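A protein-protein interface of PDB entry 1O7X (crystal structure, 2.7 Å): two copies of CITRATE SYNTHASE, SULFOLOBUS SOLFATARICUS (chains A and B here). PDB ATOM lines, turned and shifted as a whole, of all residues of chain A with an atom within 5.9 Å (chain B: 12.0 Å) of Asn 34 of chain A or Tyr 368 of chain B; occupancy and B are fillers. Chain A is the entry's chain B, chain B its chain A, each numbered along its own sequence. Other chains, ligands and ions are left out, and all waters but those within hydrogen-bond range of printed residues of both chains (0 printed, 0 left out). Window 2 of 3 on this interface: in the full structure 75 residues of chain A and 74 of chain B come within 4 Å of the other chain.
Of the 12 printed residues of chain A, 4 touch a printed residue of chain B. Hydrophobic or aromatic side chains of chain A within 4 Å of the printed part of chain B: Tyr 33. Printed residues of chain B that touch a printed residue of chain A: Tyr 363, Pro 366, Glu 367, Tyr 368 and Gln 369. Among the printed residues, 8 pairs touch across the chains.
Asn 34 of chain A touches just one residue of chain B: Tyr 368. Tyr 368 of chain B touches three residues of chain A. No residue of chain B comes within 4 Å of Ile 27 of chain A. No residue of chain B comes within 4 Å of Leu 28 of chain A. Of chain B, only Glu 367 (3.5 Å) and Tyr 368 (3.1 Å) come within 4 Å of Arg 29 of chain A. No residue of chain B comes within 4 Å of Glu 36 of chain A. No residue of chain B comes within 4 Å of Asp 37 of chain A. No residue of chain B comes within 4 Å of Leu 38 of chain A. Of the printed residues of chain A, Gln 369 of chain B touches Gly 32 and Tyr 33. Of the printed residues of chain A, Tyr 363 of chain B touches Gly 32. Printed residues of chain A within 4 Å of Glu 367 of chain B: Arg 29. Printed residues of chain A within 4 Å of Pro 366 of chain B: Gly 32. Val 39 of chain A touches none of the printed residues of chain B.
No position is printed for both chains.
The guanidinium group (NH1) of Arg 29 of chain A lies within hydrogen-bond range of the backbone carbonyl oxygen (O) of Glu 367 of chain B (3.5 Å). The backbone carbonyl oxygen (O) of Gly 32 of chain A sits at hydrogen-bond distance from the backbone NH (N) of Gln 369 of chain B (3.1 Å). The side-chain amide oxygen (OE1) of Gln 369 of chain B sits close to the side-chain hydroxyl (OH) of Tyr 33 of chain A (3.2 Å).
Among the printed residues, pairs that only touch across the chains: Arg 29 of chain A with Tyr 368 of chain B, Asn 34 of chain A with Tyr 368 of chain B, Gly 32 of chain A with Tyr 368 of chain B, Gly 32 of chain A with Tyr 363 of chain B and Gly 32 of chain A with Pro 366 of chain B.
The side-chain hydroxyl of Tyr 363 of chain B lies within hydrogen-bond range of the backbone carbonyl oxygen of Pro 366 of chain B, 2.8 Å away. OD1 of Asn 34 of chain A sits at hydrogen-bond distance from NE of Arg 29 of chain A.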
ATOM      1  N   ILE A  27      24.219   5.322 -33.111  1.00  0.00           N
ATOM      2  CA  ILE A  27      23.936   5.185 -31.689  1.00  0.00           C
ATOM      3  C   ILE A  27      25.115   5.636 -30.844  1.00  0.00           C
ATOM      4  O   ILE A  27      26.217   5.148 -31.068  1.00  0.00           O
ATOM      5  CB  ILE A  27      23.572   3.730 -31.347  1.00  0.00           C
ATOM      6  CG1 ILE A  27      22.150   3.433 -31.836  1.00  0.00           C
ATOM      7  CG2 ILE A  27      23.787   3.435 -29.872  1.00  0.00           C
ATOM      8  CD1 ILE A  27      21.039   3.449 -30.817  1.00  0.00           C
ATOM      9  N   LEU A  28      24.860   6.487 -29.855  1.00  0.00           N
ATOM     10  CA  LEU A  28      25.909   6.925 -28.955  1.00  0.00           C
ATOM     11  C   LEU A  28      25.527   6.510 -27.553  1.00  0.00           C
ATOM     12  O   LEU A  28      24.439   6.836 -27.086  1.00  0.00           O
ATOM     13  CB  LEU A  28      26.116   8.435 -29.065  1.00  0.00           C
ATOM     14  CG  LEU A  28      26.742   9.112 -27.844  1.00  0.00           C
ATOM     15  CD1 LEU A  28      28.195   8.691 -27.646  1.00  0.00           C
ATOM     16  CD2 LEU A  28      26.601  10.622 -27.938  1.00  0.00           C
ATOM     17  N   ARG A  29      26.363   5.772 -26.841  1.00  0.00           N
ATOM     18  CA  ARG A  29      26.065   5.393 -25.466  1.00  0.00           C
ATOM     19  C   ARG A  29      27.192   5.775 -24.515  1.00  0.00           C
ATOM     20  O   ARG A  29      28.352   5.837 -24.912  1.00  0.00           O
ATOM     21  CB  ARG A  29      25.811   3.900 -25.376  1.00  0.00           C
ATOM     22  CG  ARG A  29      24.604   3.406 -26.146  1.00  0.00           C
ATOM     23  CD  ARG A  29      24.446   1.903 -25.954  1.00  0.00           C
ATOM     24  NE  ARG A  29      23.103   1.583 -26.364  1.00  0.00           N
ATOM     25  CZ  ARG A  29      22.756   0.668 -27.255  1.00  0.00           C
ATOM     26  NH1 ARG A  29      23.740  -0.037 -27.807  1.00  0.00           N
ATOM     27  NH2 ARG A  29      21.465   0.522 -27.548  1.00  0.00           N
ATOM     28  N   TYR A  30      26.836   6.078 -23.281  1.00  0.00           N
ATOM     29  CA  TYR A  30      27.706   6.426 -22.182  1.00  0.00           C
ATOM     30  C   TYR A  30      27.546   5.368 -21.094  1.00  0.00           C
ATOM     31  O   TYR A  30      26.447   5.290 -20.536  1.00  0.00           O
ATOM     32  CB  TYR A  30      27.293   7.740 -21.549  1.00  0.00           C
ATOM     33  CG  TYR A  30      27.532   9.009 -22.314  1.00  0.00           C
ATOM     34  CD1 TYR A  30      26.925  10.208 -21.949  1.00  0.00           C
ATOM     35  CD2 TYR A  30      28.391   9.014 -23.396  1.00  0.00           C
ATOM     36  CE1 TYR A  30      27.173  11.371 -22.646  1.00  0.00           C
ATOM     37  CE2 TYR A  30      28.650  10.184 -24.093  1.00  0.00           C
ATOM     38  CZ  TYR A  30      28.039  11.351 -23.719  1.00  0.00           C
ATOM     39  OH  TYR A  30      28.343  12.455 -24.457  1.00  0.00           O
ATOM     40  N   GLY A  32      26.773   2.298 -21.538  1.00  0.00           N
ATOM     41  CA  GLY A  32      25.643   1.452 -21.861  1.00  0.00           C
ATOM     42  C   GLY A  32      24.289   2.106 -22.085  1.00  0.00           C
ATOM     43  O   GLY A  32      23.407   1.587 -22.787  1.00  0.00           O
ATOM     44  N   TYR A  33      24.080   3.283 -21.509  1.00  0.00           N
ATOM     45  CA  TYR A  33      22.863   4.044 -21.637  1.00  0.00           C
ATOM     46  C   TYR A  33      22.761   4.798 -22.929  1.00  0.00           C
ATOM     47  O   TYR A  33      23.688   5.591 -23.119  1.00  0.00           O
ATOM     48  CB  TYR A  33      22.858   5.012 -20.416  1.00  0.00           C
ATOM     49  CG  TYR A  33      22.723   4.199 -19.137  1.00  0.00           C
ATOM     50  CD1 TYR A  33      23.787   4.038 -18.261  1.00  0.00           C
ATOM     51  CD2 TYR A  33      21.516   3.531 -18.867  1.00  0.00           C
ATOM     52  CE1 TYR A  33      23.634   3.293 -17.105  1.00  0.00           C
ATOM     53  CE2 TYR A  33      21.391   2.743 -17.750  1.00  0.00           C
ATOM     54  CZ  TYR A  33      22.457   2.605 -16.881  1.00  0.00           C
ATOM     55  OH  TYR A  33      22.303   1.817 -15.755  1.00  0.00           O
ATOM     56  N   ASN A  34      21.755   4.748 -23.779  1.00  0.00           N
ATOM     57  CA  ASN A  34      21.685   5.657 -24.920  1.00  0.00           C
ATOM     58  C   ASN A  34      21.585   7.125 -24.498  1.00  0.00           C
ATOM     59  O   ASN A  34      20.911   7.471 -23.511  1.00  0.00           O
ATOM     60  CB  ASN A  34      20.419   5.391 -25.752  1.00  0.00           C
ATOM     61  CG  ASN A  34      20.486   3.989 -26.319  1.00  0.00           C
ATOM     62  OD1 ASN A  34      21.475   3.676 -27.008  1.00  0.00           O
ATOM     63  ND2 ASN A  34      19.512   3.117 -26.072  1.00  0.00           N
ATOM     64  N   ILE A  35      22.213   8.005 -25.315  1.00  0.00           N
ATOM     65  CA  ILE A  35      22.163   9.417 -25.009  1.00  0.00           C
ATOM     66  C   ILE A  35      20.703   9.917 -24.939  1.00  0.00           C
ATOM     67  O   ILE A  35      20.459  10.790 -24.113  1.00  0.00           O
ATOM     68  CB  ILE A  35      22.811  10.458 -25.942  1.00  0.00           C
ATOM     69  CG1 ILE A  35      22.855   9.980 -27.388  1.00  0.00           C
ATOM     70  CG2 ILE A  35      24.112  10.993 -25.386  1.00  0.00           C
ATOM     71  CD1 ILE A  35      22.647  11.160 -28.336  1.00  0.00           C
ATOM     72  N   GLU A  36      19.866   9.472 -25.848  1.00  0.00           N
ATOM     73  CA  GLU A  36      18.459   9.842 -25.885  1.00  0.00           C
ATOM     74  C   GLU A  36      17.775   9.575 -24.557  1.00  0.00           C
ATOM     75  O   GLU A  36      17.040  10.485 -24.198  1.00  0.00           O
ATOM     76  CB  GLU A  36      17.683   9.141 -26.999  1.00  0.00           C
ATOM     77  CG  GLU A  36      18.702   8.354 -27.844  1.00  0.00           C
ATOM     78  CD  GLU A  36      18.457   8.590 -29.315  1.00  0.00           C
ATOM     79  OE1 GLU A  36      17.238   8.721 -29.614  1.00  0.00           O
ATOM     80  OE2 GLU A  36      19.459   8.623 -30.065  1.00  0.00           O
ATOM     81  N   ASP A  37      18.036   8.498 -23.846  1.00  0.00           N
ATOM     82  CA  ASP A  37      17.468   8.266 -22.539  1.00  0.00           C
ATOM     83  C   ASP A  37      17.992   9.306 -21.547  1.00  0.00           C
ATOM     84  O   ASP A  37      17.276   9.768 -20.665  1.00  0.00           O
ATOM     85  CB  ASP A  37      17.843   6.884 -21.989  1.00  0.00           C
ATOM     86  CG  ASP A  37      17.183   5.761 -22.731  1.00  0.00           C
ATOM     87  OD1 ASP A  37      16.042   5.971 -23.178  1.00  0.00           O
ATOM     88  OD2 ASP A  37      17.713   4.643 -22.904  1.00  0.00           O
ATOM     89  N   LEU A  38      19.288   9.611 -21.600  1.00  0.00           N
ATOM     90  CA  LEU A  38      19.896  10.590 -20.715  1.00  0.00           C
ATOM     91  C   LEU A  38      19.280  11.975 -20.912  1.00  0.00           C
ATOM     92  O   LEU A  38      18.921  12.649 -19.940  1.00  0.00           O
ATOM     93  CB  LEU A  38      21.396  10.607 -20.994  1.00  0.00           C
ATOM     94  CG  LEU A  38      22.300   9.422 -20.694  1.00  0.00           C
ATOM     95  CD1 LEU A  38      23.695   9.887 -20.302  1.00  0.00           C
ATOM     96  CD2 LEU A  38      21.764   8.488 -19.618  1.00  0.00           C
ATOM     97  N   VAL A  39      19.137  12.412 -22.180  1.00  0.00           N
ATOM     98  CA  VAL A  39      18.551  13.713 -22.435  1.00  0.00           C
ATOM     99  C   VAL A  39      17.040  13.686 -22.176  1.00  0.00           C
ATOM    100  O   VAL A  39      16.506  14.670 -21.669  1.00  0.00           O
ATOM    101  CB  VAL A  39      18.829  14.324 -23.819  1.00  0.00           C
ATOM    102  CG1 VAL A  39      20.254  14.096 -24.261  1.00  0.00           C
ATOM    103  CG2 VAL A  39      17.863  13.806 -24.867  1.00  0.00           C
ATOM    104  N   TYR B 363      36.394  -0.097 -26.779  1.00  0.00           N
ATOM    105  CA  TYR B 363      35.293  -0.084 -25.840  1.00  0.00           C
ATOM    106  C   TYR B 363      34.960  -1.479 -25.336  1.00  0.00           C
ATOM    107  O   TYR B 363      34.499  -2.323 -26.076  1.00  0.00           O
ATOM    108  CB  TYR B 363      34.012   0.500 -26.505  1.00  0.00           C
ATOM    109  CG  TYR B 363      32.868   0.501 -25.510  1.00  0.00           C
ATOM    110  CD1 TYR B 363      32.863   1.431 -24.494  1.00  0.00           C
ATOM    111  CD2 TYR B 363      31.860  -0.450 -25.540  1.00  0.00           C
ATOM    112  CE1 TYR B 363      31.859   1.430 -23.533  1.00  0.00           C
ATOM    113  CE2 TYR B 363      30.854  -0.459 -24.604  1.00  0.00           C
ATOM    114  CZ  TYR B 363      30.864   0.488 -23.614  1.00  0.00           C
ATOM    115  OH  TYR B 363      29.878   0.525 -22.657  1.00  0.00           O
ATOM    116  N   VAL B 364      35.260  -1.756 -24.105  1.00  0.00           N
ATOM    117  CA  VAL B 364      34.917  -3.022 -23.429  1.00  0.00           C
ATOM    118  C   VAL B 364      33.759  -2.542 -22.581  1.00  0.00           C
ATOM    119  O   VAL B 364      33.379  -1.379 -22.942  1.00  0.00           O
ATOM    120  CB  VAL B 364      36.146  -3.521 -22.686  1.00  0.00           C
ATOM    121  CG1 VAL B 364      37.265  -3.681 -23.723  1.00  0.00           C
ATOM    122  CG2 VAL B 364      36.614  -2.563 -21.630  1.00  0.00           C
ATOM    123  N   GLY B 365      33.174  -3.099 -21.545  1.00  0.00           N
ATOM    124  CA  GLY B 365      32.072  -2.278 -20.958  1.00  0.00           C
ATOM    125  C   GLY B 365      30.706  -2.607 -21.538  1.00  0.00           C
ATOM    126  O   GLY B 365      30.582  -2.995 -22.689  1.00  0.00           O
ATOM    127  N   PRO B 366      29.671  -2.447 -20.723  1.00  0.00           N
ATOM    128  CA  PRO B 366      28.291  -2.798 -20.996  1.00  0.00           C
ATOM    129  C   PRO B 366      27.807  -2.510 -22.397  1.00  0.00           C
ATOM    130  O   PRO B 366      27.978  -1.441 -22.953  1.00  0.00           O
ATOM    131  CB  PRO B 366      27.456  -2.039 -19.971  1.00  0.00           C
ATOM    132  CG  PRO B 366      28.417  -1.258 -19.160  1.00  0.00           C
ATOM    133  CD  PRO B 366      29.767  -1.915 -19.331  1.00  0.00           C
ATOM    134  N   GLU B 367      27.199  -3.521 -22.999  1.00  0.00           N
ATOM    135  CA  GLU B 367      26.720  -3.395 -24.379  1.00  0.00           C
ATOM    136  C   GLU B 367      25.561  -2.407 -24.412  1.00  0.00           C
ATOM    137  O   GLU B 367      25.555  -1.447 -25.184  1.00  0.00           O
ATOM    138  CB  GLU B 367      26.402  -4.782 -24.916  1.00  0.00           C
ATOM    139  CG  GLU B 367      25.662  -4.769 -26.247  1.00  0.00           C
ATOM    140  CD  GLU B 367      25.474  -6.173 -26.796  1.00  0.00           C
ATOM    141  OE1 GLU B 367      25.683  -7.117 -25.998  1.00  0.00           O
ATOM    142  OE2 GLU B 367      25.128  -6.304 -27.988  1.00  0.00           O
ATOM    143  N   TYR B 368      24.613  -2.603 -23.514  1.00  0.00           N
ATOM    144  CA  TYR B 368      23.458  -1.740 -23.371  1.00  0.00           C
ATOM    145  C   TYR B 368      22.892  -1.899 -21.966  1.00  0.00           C
ATOM    146  O   TYR B 368      22.245  -2.911 -21.706  1.00  0.00           O
ATOM    147  CB  TYR B 368      22.416  -2.071 -24.431  1.00  0.00           C
ATOM    148  CG  TYR B 368      21.048  -1.486 -24.194  1.00  0.00           C
ATOM    149  CD1 TYR B 368      20.725  -0.196 -24.609  1.00  0.00           C
ATOM    150  CD2 TYR B 368      20.062  -2.225 -23.550  1.00  0.00           C
ATOM    151  CE1 TYR B 368      19.464   0.333 -24.403  1.00  0.00           C
ATOM    152  CE2 TYR B 368      18.800  -1.696 -23.327  1.00  0.00           C
ATOM    153  CZ  TYR B 368      18.508  -0.421 -23.759  1.00  0.00           C
ATOM    154  OH  TYR B 368      17.245   0.083 -23.534  1.00  0.00           O
ATOM    155  N   GLN B 369      23.163  -0.964 -21.069  1.00  0.00           N
ATOM    156  CA  GLN B 369      22.632  -1.012 -19.716  1.00  0.00           C
ATOM    157  C   GLN B 369      21.256  -0.346 -19.822  1.00  0.00           C
ATOM    158  O   GLN B 369      20.870   0.123 -20.891  1.00  0.00           O
ATOM    159  CB  GLN B 369      23.465  -0.321 -18.658  1.00  0.00           C
ATOM    160  CG  GLN B 369      24.604  -1.057 -18.000  1.00  0.00           C
ATOM    161  CD  GLN B 369      25.535  -0.239 -17.142  1.00  0.00           C
ATOM    162  OE1 GLN B 369      25.258   0.852 -16.644  1.00  0.00           O
ATOM    163  NE2 GLN B 369      26.769  -0.680 -16.842  1.00  0.00           N
